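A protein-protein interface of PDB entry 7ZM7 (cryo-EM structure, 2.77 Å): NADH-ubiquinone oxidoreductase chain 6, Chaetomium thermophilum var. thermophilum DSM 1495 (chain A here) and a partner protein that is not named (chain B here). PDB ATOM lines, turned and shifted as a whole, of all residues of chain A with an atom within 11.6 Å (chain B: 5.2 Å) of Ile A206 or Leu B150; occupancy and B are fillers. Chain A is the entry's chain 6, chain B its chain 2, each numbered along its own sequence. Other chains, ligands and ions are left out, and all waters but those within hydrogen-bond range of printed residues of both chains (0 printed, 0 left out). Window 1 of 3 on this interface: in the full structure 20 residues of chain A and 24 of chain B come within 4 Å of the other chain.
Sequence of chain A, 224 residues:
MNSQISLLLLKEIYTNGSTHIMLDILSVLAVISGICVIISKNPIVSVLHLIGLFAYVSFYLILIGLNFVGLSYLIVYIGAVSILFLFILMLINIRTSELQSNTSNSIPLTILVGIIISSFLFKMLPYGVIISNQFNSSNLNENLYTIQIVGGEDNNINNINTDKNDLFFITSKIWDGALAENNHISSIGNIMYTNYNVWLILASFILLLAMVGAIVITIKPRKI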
ATOM      1  N   MET A 192       8.010  19.454  22.257  1.00  0.00           N
ATOM      2  CA  MET A 192       7.218  18.251  22.029  1.00  0.00           C
ATOM      3  C   MET A 192       8.012  16.973  22.279  1.00  0.00           C
ATOM      4  O   MET A 192       7.431  15.932  22.605  1.00  0.00           O
ATOM      5  CB  MET A 192       6.676  18.293  20.604  1.00  0.00           C
ATOM      6  CG  MET A 192       6.307  16.988  19.980  1.00  0.00           C
ATOM      7  SD  MET A 192       5.552  17.182  18.374  1.00  0.00           S
ATOM      8  CE  MET A 192       4.664  15.640  18.326  1.00  0.00           C
ATOM      9  N   TYR A 196       7.718  17.701  27.414  1.00  0.00           N
ATOM     10  CA  TYR A 196       6.384  17.061  27.512  1.00  0.00           C
ATOM     11  C   TYR A 196       6.415  15.732  26.753  1.00  0.00           C
ATOM     12  O   TYR A 196       5.377  15.355  26.204  1.00  0.00           O
ATOM     13  CB  TYR A 196       5.298  18.041  27.072  1.00  0.00           C
ATOM     14  CG  TYR A 196       5.190  19.322  27.858  1.00  0.00           C
ATOM     15  CD1 TYR A 196       5.926  20.442  27.509  1.00  0.00           C
ATOM     16  CD2 TYR A 196       4.337  19.420  28.940  1.00  0.00           C
ATOM     17  CE1 TYR A 196       5.833  21.619  28.229  1.00  0.00           C
ATOM     18  CE2 TYR A 196       4.224  20.592  29.667  1.00  0.00           C
ATOM     19  CZ  TYR A 196       4.977  21.695  29.312  1.00  0.00           C
ATOM     20  OH  TYR A 196       4.867  22.848  30.029  1.00  0.00           O
ATOM     21  N   ASN A 197       7.561  15.041  26.738  1.00  0.00           N
ATOM     22  CA  ASN A 197       7.725  13.802  25.923  1.00  0.00           C
ATOM     23  C   ASN A 197       6.871  12.635  26.422  1.00  0.00           C
ATOM     24  O   ASN A 197       6.735  11.669  25.666  1.00  0.00           O
ATOM     25  CB  ASN A 197       9.196  13.415  25.733  1.00  0.00           C
ATOM     26  CG  ASN A 197       9.939  13.084  27.010  1.00  0.00           C
ATOM     27  OD1 ASN A 197       9.364  13.069  28.095  1.00  0.00           O
ATOM     28  ND2 ASN A 197      11.228  12.817  26.887  1.00  0.00           N
ATOM     29  N   VAL A 198       6.352  12.701  27.647  1.00  0.00           N
ATOM     30  CA  VAL A 198       5.432  11.633  28.148  1.00  0.00           C
ATOM     31  C   VAL A 198       4.163  11.648  27.291  1.00  0.00           C
ATOM     32  O   VAL A 198       3.622  10.564  27.018  1.00  0.00           O
ATOM     33  CB  VAL A 198       5.167  11.758  29.664  1.00  0.00           C
ATOM     34  CG1 VAL A 198       3.748  11.381  30.066  1.00  0.00           C
ATOM     35  CG2 VAL A 198       6.181  10.962  30.466  1.00  0.00           C
ATOM     36  N   TRP A 199       3.703  12.834  26.890  1.00  0.00           N
ATOM     37  CA  TRP A 199       2.515  12.931  25.998  1.00  0.00           C
ATOM     38  C   TRP A 199       2.797  12.221  24.672  1.00  0.00           C
ATOM     39  O   TRP A 199       1.858  11.641  24.123  1.00  0.00           O
ATOM     40  CB  TRP A 199       2.097  14.385  25.771  1.00  0.00           C
ATOM     41  CG  TRP A 199       1.611  15.098  26.993  1.00  0.00           C
ATOM     42  CD1 TRP A 199       1.223  14.546  28.178  1.00  0.00           C
ATOM     43  CD2 TRP A 199       1.447  16.518  27.138  1.00  0.00           C
ATOM     44  NE1 TRP A 199       0.838  15.525  29.052  1.00  0.00           N
ATOM     45  CE2 TRP A 199       0.965  16.745  28.443  1.00  0.00           C
ATOM     46  CE3 TRP A 199       1.659  17.613  26.296  1.00  0.00           C
ATOM     47  CZ2 TRP A 199       0.697  18.024  28.922  1.00  0.00           C
ATOM     48  CZ3 TRP A 199       1.391  18.877  26.770  1.00  0.00           C
ATOM     49  CH2 TRP A 199       0.915  19.076  28.065  1.00  0.00           C
ATOM     50  N   LEU A 200       4.043  12.260  24.186  1.00  0.00           N
ATOM     51  CA  LEU A 200       4.374  11.544  22.964  1.00  0.00           C
ATOM     52  C   LEU A 200       4.342  10.038  23.184  1.00  0.00           C
ATOM     53  O   LEU A 200       3.970   9.286  22.283  1.00  0.00           O
ATOM     54  CB  LEU A 200       5.742  12.002  22.459  1.00  0.00           C
ATOM     55  CG  LEU A 200       6.177  11.669  21.032  1.00  0.00           C
ATOM     56  CD1 LEU A 200       5.255  12.221  19.972  1.00  0.00           C
ATOM     57  CD2 LEU A 200       7.559  12.190  20.843  1.00  0.00           C
ATOM     58  N   ILE A 201       4.740   9.580  24.368  1.00  0.00           N
ATOM     59  CA  ILE A 201       4.730   8.151  24.658  1.00  0.00           C
ATOM     60  C   ILE A 201       3.304   7.605  24.662  1.00  0.00           C
ATOM     61  O   ILE A 201       3.018   6.582  24.038  1.00  0.00           O
ATOM     62  CB  ILE A 201       5.447   7.866  25.987  1.00  0.00           C
ATOM     63  CG1 ILE A 201       6.884   8.359  25.926  1.00  0.00           C
ATOM     64  CG2 ILE A 201       5.418   6.389  26.299  1.00  0.00           C
ATOM     65  CD1 ILE A 201       7.692   7.697  24.872  1.00  0.00           C
ATOM     66  N   LEU A 202       2.391   8.278  25.360  1.00  0.00           N
ATOM     67  CA  LEU A 202       1.011   7.813  25.411  1.00  0.00           C
ATOM     68  C   LEU A 202       0.385   7.813  24.033  1.00  0.00           C
ATOM     69  O   LEU A 202      -0.374   6.903  23.688  1.00  0.00           O
ATOM     70  CB  LEU A 202       0.184   8.689  26.346  1.00  0.00           C
ATOM     71  CG  LEU A 202       0.334   8.604  27.864  1.00  0.00           C
ATOM     72  CD1 LEU A 202       0.006   9.959  28.471  1.00  0.00           C
ATOM     73  CD2 LEU A 202      -0.562   7.561  28.447  1.00  0.00           C
ATOM     74  N   ALA A 203       0.654   8.854  23.246  1.00  0.00           N
ATOM     75  CA  ALA A 203       0.079   8.941  21.916  1.00  0.00           C
ATOM     76  C   ALA A 203       0.630   7.852  21.008  1.00  0.00           C
ATOM     77  O   ALA A 203      -0.114   7.254  20.227  1.00  0.00           O
ATOM     78  CB  ALA A 203       0.337  10.319  21.336  1.00  0.00           C
ATOM     79  N   SER A 204       1.926   7.577  21.104  1.00  0.00           N
ATOM     80  CA  SER A 204       2.501   6.466  20.360  1.00  0.00           C
ATOM     81  C   SER A 204       1.802   5.161  20.695  1.00  0.00           C
ATOM     82  O   SER A 204       1.651   4.289  19.835  1.00  0.00           O
ATOM     83  CB  SER A 204       3.990   6.357  20.666  1.00  0.00           C
ATOM     84  OG  SER A 204       4.183   5.972  22.012  1.00  0.00           O
ATOM     85  N   PHE A 205       1.386   5.001  21.943  1.00  0.00           N
ATOM     86  CA  PHE A 205       0.729   3.773  22.337  1.00  0.00           C
ATOM     87  C   PHE A 205      -0.745   3.750  21.950  1.00  0.00           C
ATOM     88  O   PHE A 205      -1.286   2.670  21.713  1.00  0.00           O
ATOM     89  CB  PHE A 205       0.921   3.548  23.834  1.00  0.00           C
ATOM     90  CG  PHE A 205       2.195   2.832  24.166  1.00  0.00           C
ATOM     91  CD1 PHE A 205       2.299   1.468  24.005  1.00  0.00           C
ATOM     92  CD2 PHE A 205       3.296   3.524  24.611  1.00  0.00           C
ATOM     93  CE1 PHE A 205       3.462   0.811  24.302  1.00  0.00           C
ATOM     94  CE2 PHE A 205       4.473   2.871  24.893  1.00  0.00           C
ATOM     95  CZ  PHE A 205       4.552   1.512  24.743  1.00  0.00           C
ATOM     96  N   ILE A 206      -1.401   4.910  21.868  1.00  0.00           N
ATOM     97  CA  ILE A 206      -2.790   4.956  21.420  1.00  0.00           C
ATOM     98  C   ILE A 206      -2.874   4.624  19.941  1.00  0.00           C
ATOM     99  O   ILE A 206      -3.740   3.860  19.511  1.00  0.00           O
ATOM    100  CB  ILE A 206      -3.420   6.329  21.723  1.00  0.00           C
ATOM    101  CG1 ILE A 206      -3.752   6.466  23.205  1.00  0.00           C
ATOM    102  CG2 ILE A 206      -4.676   6.541  20.919  1.00  0.00           C
ATOM    103  CD1 ILE A 206      -4.280   7.819  23.587  1.00  0.00           C
ATOM    104  N   LEU A 207      -1.973   5.195  19.140  1.00  0.00           N
ATOM    105  CA  LEU A 207      -1.923   4.878  17.718  1.00  0.00           C
ATOM    106  C   LEU A 207      -1.562   3.419  17.488  1.00  0.00           C
ATOM    107  O   LEU A 207      -2.087   2.775  16.576  1.00  0.00           O
ATOM    108  CB  LEU A 207      -0.915   5.789  17.022  1.00  0.00           C
ATOM    109  CG  LEU A 207      -1.117   7.300  17.122  1.00  0.00           C
ATOM    110  CD1 LEU A 207       0.217   8.016  16.999  1.00  0.00           C
ATOM    111  CD2 LEU A 207      -2.061   7.790  16.067  1.00  0.00           C
ATOM    112  N   LEU A 208      -0.642   2.891  18.287  1.00  0.00           N
ATOM    113  CA  LEU A 208      -0.243   1.496  18.175  1.00  0.00           C
ATOM    114  C   LEU A 208      -1.385   0.551  18.539  1.00  0.00           C
ATOM    115  O   LEU A 208      -1.508  -0.532  17.964  1.00  0.00           O
ATOM    116  CB  LEU A 208       0.973   1.253  19.067  1.00  0.00           C
ATOM    117  CG  LEU A 208       1.496  -0.159  19.246  1.00  0.00           C
ATOM    118  CD1 LEU A 208       2.064  -0.638  17.956  1.00  0.00           C
ATOM    119  CD2 LEU A 208       2.549  -0.166  20.289  1.00  0.00           C
ATOM    120  N   LEU A 209      -2.214   0.931  19.511  1.00  0.00           N
ATOM    121  CA  LEU A 209      -3.380   0.128  19.851  1.00  0.00           C
ATOM    122  C   LEU A 209      -4.441   0.195  18.755  1.00  0.00           C
ATOM    123  O   LEU A 209      -5.088  -0.810  18.452  1.00  0.00           O
ATOM    124  CB  LEU A 209      -3.949   0.580  21.194  1.00  0.00           C
ATOM    125  CG  LEU A 209      -5.348   0.085  21.574  1.00  0.00           C
ATOM    126  CD1 LEU A 209      -5.307  -1.359  21.985  1.00  0.00           C
ATOM    127  CD2 LEU A 209      -5.968   0.941  22.666  1.00  0.00           C
ATOM    128  N   ALA A 210      -4.635   1.362  18.155  1.00  0.00           N
ATOM    129  CA  ALA A 210      -5.576   1.486  17.056  1.00  0.00           C
ATOM    130  C   ALA A 210      -5.114   0.747  15.810  1.00  0.00           C
ATOM    131  O   ALA A 210      -5.927   0.487  14.925  1.00  0.00           O
ATOM    132  CB  ALA A 210      -5.817   2.962  16.751  1.00  0.00           C
ATOM    133  N   MET A 211      -3.828   0.419  15.713  1.00  0.00           N
ATOM    134  CA  MET A 211      -3.353  -0.437  14.634  1.00  0.00           C
ATOM    135  C   MET A 211      -3.688  -1.891  14.911  1.00  0.00           C
ATOM    136  O   MET A 211      -4.383  -2.542  14.131  1.00  0.00           O
ATOM    137  CB  MET A 211      -1.848  -0.268  14.456  1.00  0.00           C
ATOM    138  CG  MET A 211      -1.239  -1.191  13.421  1.00  0.00           C
ATOM    139  SD  MET A 211      -1.429  -0.559  11.747  1.00  0.00           S
ATOM    140  CE  MET A 211      -0.017   0.534  11.650  1.00  0.00           C
ATOM    141  N   VAL A 212      -3.215  -2.405  16.039  1.00  0.00           N
ATOM    142  CA  VAL A 212      -3.379  -3.815  16.363  1.00  0.00           C
ATOM    143  C   VAL A 212      -4.850  -4.163  16.516  1.00  0.00           C
ATOM    144  O   VAL A 212      -5.314  -5.187  16.009  1.00  0.00           O
ATOM    145  CB  VAL A 212      -2.586  -4.144  17.636  1.00  0.00           C
ATOM    146  CG1 VAL A 212      -2.973  -5.494  18.193  1.00  0.00           C
ATOM    147  CG2 VAL A 212      -1.109  -4.066  17.345  1.00  0.00           C
ATOM    148  N   GLY A 213      -5.601  -3.321  17.222  1.00  0.00           N
ATOM    149  CA  GLY A 213      -6.981  -3.647  17.514  1.00  0.00           C
ATOM    150  C   GLY A 213      -7.873  -3.637  16.292  1.00  0.00           C
ATOM    151  O   GLY A 213      -8.766  -4.472  16.159  1.00  0.00           O
ATOM    152  N   ALA A 214      -7.684  -2.671  15.409  1.00  0.00           N
ATOM    153  CA  ALA A 214      -8.561  -2.587  14.251  1.00  0.00           C
ATOM    154  C   ALA A 214      -8.216  -3.634  13.206  1.00  0.00           C
ATOM    155  O   ALA A 214      -9.102  -4.109  12.492  1.00  0.00           O
ATOM    156  CB  ALA A 214      -8.501  -1.183  13.664  1.00  0.00           C
ATOM    157  N   ILE A 215      -6.946  -4.016  13.112  1.00  0.00           N
ATOM    158  CA  ILE A 215      -6.568  -5.122  12.246  1.00  0.00           C
ATOM    159  C   ILE A 215      -7.127  -6.436  12.782  1.00  0.00           C
ATOM    160  O   ILE A 215      -7.633  -7.260  12.018  1.00  0.00           O
ATOM    161  CB  ILE A 215      -5.036  -5.158  12.073  1.00  0.00           C
ATOM    162  CG1 ILE A 215      -4.597  -4.051  11.111  1.00  0.00           C
ATOM    163  CG2 ILE A 215      -4.572  -6.506  11.555  1.00  0.00           C
ATOM    164  CD1 ILE A 215      -3.104  -3.794  11.080  1.00  0.00           C
ATOM    165  N   LEU B 145      -3.977  17.694  32.680  1.00  0.00           N
ATOM    166  CA  LEU B 145      -5.244  17.461  31.949  1.00  0.00           C
ATOM    167  C   LEU B 145      -4.931  16.603  30.732  1.00  0.00           C
ATOM    168  O   LEU B 145      -5.687  15.653  30.506  1.00  0.00           O
ATOM    169  CB  LEU B 145      -5.819  18.823  31.553  1.00  0.00           C
ATOM    170  CG  LEU B 145      -6.247  19.704  32.726  1.00  0.00           C
ATOM    171  CD1 LEU B 145      -6.702  21.071  32.246  1.00  0.00           C
ATOM    172  CD2 LEU B 145      -7.329  19.035  33.551  1.00  0.00           C
ATOM    173  N   VAL B 146      -3.927  16.969  29.930  1.00  0.00           N
ATOM    174  CA  VAL B 146      -3.692  16.168  28.733  1.00  0.00           C
ATOM    175  C   VAL B 146      -3.416  14.718  29.111  1.00  0.00           C
ATOM    176  O   VAL B 146      -3.909  13.788  28.470  1.00  0.00           O
ATOM    177  CB  VAL B 146      -2.552  16.781  27.895  1.00  0.00           C
ATOM    178  CG1 VAL B 146      -2.421  16.096  26.558  1.00  0.00           C
ATOM    179  CG2 VAL B 146      -2.794  18.250  27.682  1.00  0.00           C
ATOM    180  N   SER B 147      -2.638  14.505  30.168  1.00  0.00           N
ATOM    181  CA  SER B 147      -2.322  13.150  30.589  1.00  0.00           C
ATOM    182  C   SER B 147      -3.577  12.379  30.961  1.00  0.00           C
ATOM    183  O   SER B 147      -3.704  11.198  30.634  1.00  0.00           O
ATOM    184  CB  SER B 147      -1.338  13.187  31.751  1.00  0.00           C
ATOM    185  OG  SER B 147      -0.096  13.677  31.331  1.00  0.00           O
ATOM    186  N   ILE B 148      -4.516  13.031  31.640  1.00  0.00           N
ATOM    187  CA  ILE B 148      -5.785  12.391  31.961  1.00  0.00           C
ATOM    188  C   ILE B 148      -6.501  11.980  30.690  1.00  0.00           C
ATOM    189  O   ILE B 148      -6.969  10.847  30.553  1.00  0.00           O
ATOM    190  CB  ILE B 148      -6.666  13.331  32.796  1.00  0.00           C
ATOM    191  CG1 ILE B 148      -6.039  13.589  34.150  1.00  0.00           C
ATOM    192  CG2 ILE B 148      -8.055  12.746  32.958  1.00  0.00           C
ATOM    193  CD1 ILE B 148      -6.614  14.772  34.820  1.00  0.00           C
ATOM    194  N   PHE B 149      -6.597  12.903  29.742  1.00  0.00           N
ATOM    195  CA  PHE B 149      -7.310  12.625  28.510  1.00  0.00           C
ATOM    196  C   PHE B 149      -6.659  11.482  27.750  1.00  0.00           C
ATOM    197  O   PHE B 149      -7.334  10.552  27.304  1.00  0.00           O
ATOM    198  CB  PHE B 149      -7.359  13.882  27.650  1.00  0.00           C
ATOM    199  CG  PHE B 149      -8.050  13.678  26.354  1.00  0.00           C
ATOM    200  CD1 PHE B 149      -9.407  13.461  26.317  1.00  0.00           C
ATOM    201  CD2 PHE B 149      -7.343  13.670  25.176  1.00  0.00           C
ATOM    202  CE1 PHE B 149     -10.035  13.246  25.130  1.00  0.00           C
ATOM    203  CE2 PHE B 149      -7.969  13.460  23.994  1.00  0.00           C
ATOM    204  CZ  PHE B 149      -9.315  13.254  23.966  1.00  0.00           C
ATOM    205  N   LEU B 150      -5.340  11.524  27.616  1.00  0.00           N
ATOM    206  CA  LEU B 150      -4.650  10.506  26.844  1.00  0.00           C
ATOM    207  C   LEU B 150      -4.706   9.155  27.537  1.00  0.00           C
ATOM    208  O   LEU B 150      -4.767   8.118  26.872  1.00  0.00           O
ATOM    209  CB  LEU B 150      -3.210  10.934  26.595  1.00  0.00           C
ATOM    210  CG  LEU B 150      -2.960  11.969  25.494  1.00  0.00           C
ATOM    211  CD1 LEU B 150      -1.617  12.584  25.670  1.00  0.00           C
ATOM    212  CD2 LEU B 150      -3.033  11.347  24.144  1.00  0.00           C
ATOM    213  N   SER B 151      -4.694   9.139  28.868  1.00  0.00           N
ATOM    214  CA  SER B 151      -4.831   7.879  29.588  1.00  0.00           C
ATOM    215  C   SER B 151      -6.241   7.323  29.485  1.00  0.00           C
ATOM    216  O   SER B 151      -6.418   6.129  29.244  1.00  0.00           O
ATOM    217  CB  SER B 151      -4.455   8.058  31.053  1.00  0.00           C
ATOM    218  OG  SER B 151      -3.117   8.462  31.183  1.00  0.00           O
ATOM    219  N   ILE B 152      -7.264   8.158  29.669  1.00  0.00           N
ATOM    220  CA  ILE B 152      -8.657   7.627  29.681  1.00  0.00           C
ATOM    221  C   ILE B 152      -8.956   7.028  28.308  1.00  0.00           C
ATOM    222  O   ILE B 152      -9.561   5.959  28.278  1.00  0.00           O
ATOM    223  CB  ILE B 152      -9.712   8.637  30.203  1.00  0.00           C
ATOM    224  CG1 ILE B 152     -10.940   7.929  30.776  1.00  0.00           C
ATOM    225  CG2 ILE B 152     -10.096   9.668  29.156  1.00  0.00           C
ATOM    226  CD1 ILE B 152     -10.619   6.818  31.748  1.00  0.00           C
ATOM    227  N   GLU B 153      -8.511   7.674  27.232  1.00  0.00           N
ATOM    228  CA  GLU B 153      -8.683   7.138  25.853  1.00  0.00           C
ATOM    229  C   GLU B 153      -7.909   5.831  25.670  1.00  0.00           C
ATOM    230  O   GLU B 153      -8.500   4.877  25.164  1.00  0.00           O
ATOM    231  CB  GLU B 153      -8.212   8.162  24.819  1.00  0.00           C
ATOM    232  CG  GLU B 153      -8.993   9.463  24.864  1.00  0.00           C
ATOM    233  CD  GLU B 153     -10.495   9.374  24.644  1.00  0.00           C
ATOM    234  OE1 GLU B 153     -11.220   9.050  25.605  1.00  0.00           O
ATOM    235  OE2 GLU B 153     -10.941   9.650  23.515  1.00  0.00           O
ATOM    236  N   LEU B 154      -6.662   5.774  26.126  1.00  0.00           N
ATOM    237  CA  LEU B 154      -5.913   4.498  26.059  1.00  0.00           C
ATOM    238  C   LEU B 154      -6.726   3.401  26.742  1.00  0.00           C
ATOM    239  O   LEU B 154      -6.713   2.270  26.236  1.00  0.00           O
ATOM    240  CB  LEU B 154      -4.556   4.665  26.744  1.00  0.00           C
ATOM    241  CG  LEU B 154      -3.557   3.526  26.566  1.00  0.00           C
ATOM    242  CD1 LEU B 154      -3.510   3.056  25.120  1.00  0.00           C
ATOM    243  CD2 LEU B 154      -2.177   3.960  27.028  1.00  0.00           C
ATOM    244  N   TYR B 157     -10.491   2.921  24.652  1.00  0.00           N
ATOM    245  CA  TYR B 157     -10.339   2.331  23.300  1.00  0.00           C
ATOM    246  C   TYR B 157     -10.013   0.844  23.389  1.00  0.00           C
ATOM    247  O   TYR B 157     -10.433   0.100  22.502  1.00  0.00           O
ATOM    248  CB  TYR B 157      -9.318   3.113  22.463  1.00  0.00           C
ATOM    249  CG  TYR B 157      -9.752   4.500  22.073  1.00  0.00           C
ATOM    250  CD1 TYR B 157     -11.065   4.765  21.729  1.00  0.00           C
ATOM    251  CD2 TYR B 157      -8.844   5.543  22.028  1.00  0.00           C
ATOM    252  CE1 TYR B 157     -11.470   6.036  21.363  1.00  0.00           C
ATOM    253  CE2 TYR B 157      -9.233   6.820  21.665  1.00  0.00           C
ATOM    254  CZ  TYR B 157     -10.550   7.067  21.333  1.00  0.00           C
ATOM    255  OH  TYR B 157     -10.939   8.322  20.971  1.00  0.00           O
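Of the printed residues of chain B, Trp A199 touches Val B146, Ser B147 and Leu B150. Leu A200 touches none of the printed residues of chain B. Ile A206 touches just these residues of chain B: Leu B150 (3.3 Å) and Leu B154 (3.9 Å). Of the printed residues of chain B, Leu A209 touches Leu B154 (3.9 Å) and Tyr B157 (3.998 Å). Leu B145 touches none of the printed residues of chain A. Of chain A, only Trp A199 comes within 4 Å of Val B146. Printed residues of chain A within 4 Å of Ser B147: Trp A199. No residue of chain A comes within 4 Å of Phe B149. Printed residues of chain A within 4 Å of Leu B150: Trp A199, Leu A202 and Ile A206. Of chain A, only Leu A202 comes within 4 Å of Ser B151. No residue of chain A comes within 4 Å of Glu B153. Leu B154 touches two residues of chain A. The nearest residue of chain A that does not touch Leu B150 is Ala A203 (4.5 Å). The nearest printed residue of chain B that does not touch Trp A199 is Leu B145 (6.0 Å).
CE2 of Trp A199 touches CB of Val B146, 3.6 Å away. Leu B150 touches Trp A199 (CD1 to O, 3.9 Å). CB of Leu B150 touches CD1 of Leu A202, at 3.8 Å. Leu A202 touches Ser B151. CD1 of Ile A206 touches O of Leu B150 (3.3 Å). Leu B154 touches Ile A206 (CD1 to CG1, 3.9 Å). Leu A209 touches Leu B154. CD2 of Leu A209 touches CB of Tyr B157, 3.998 Å away.
The indole nitrogen (NE1) of Trp A199 sits at hydrogen-bond distance from the side-chain hydroxyl (OG) of Ser B147 (3.1 Å).
Of the 21 printed residues of chain A, 4 touch a printed residue of chain B. Hydrophobic or aromatic side chains of chain B that line the printed part of chain A: Val B146, Leu B150, Leu B154 and Tyr B157. Among the printed residues, 9 pairs touch across the chains. Among the printed residues, no Asp or Glu carboxylate lies within 4 Å of a Lys or Arg side-chain nitrogen of the other chain.
O of Ser B147 lies within hydrogen-bond range of OG of Ser B151 (2.9 Å). The side-chain hydroxyl (OH) of Tyr B157 sits at hydrogen-bond distance from the side-chain carboxylate (OE2) of Glu B153, at 2.9 Å.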
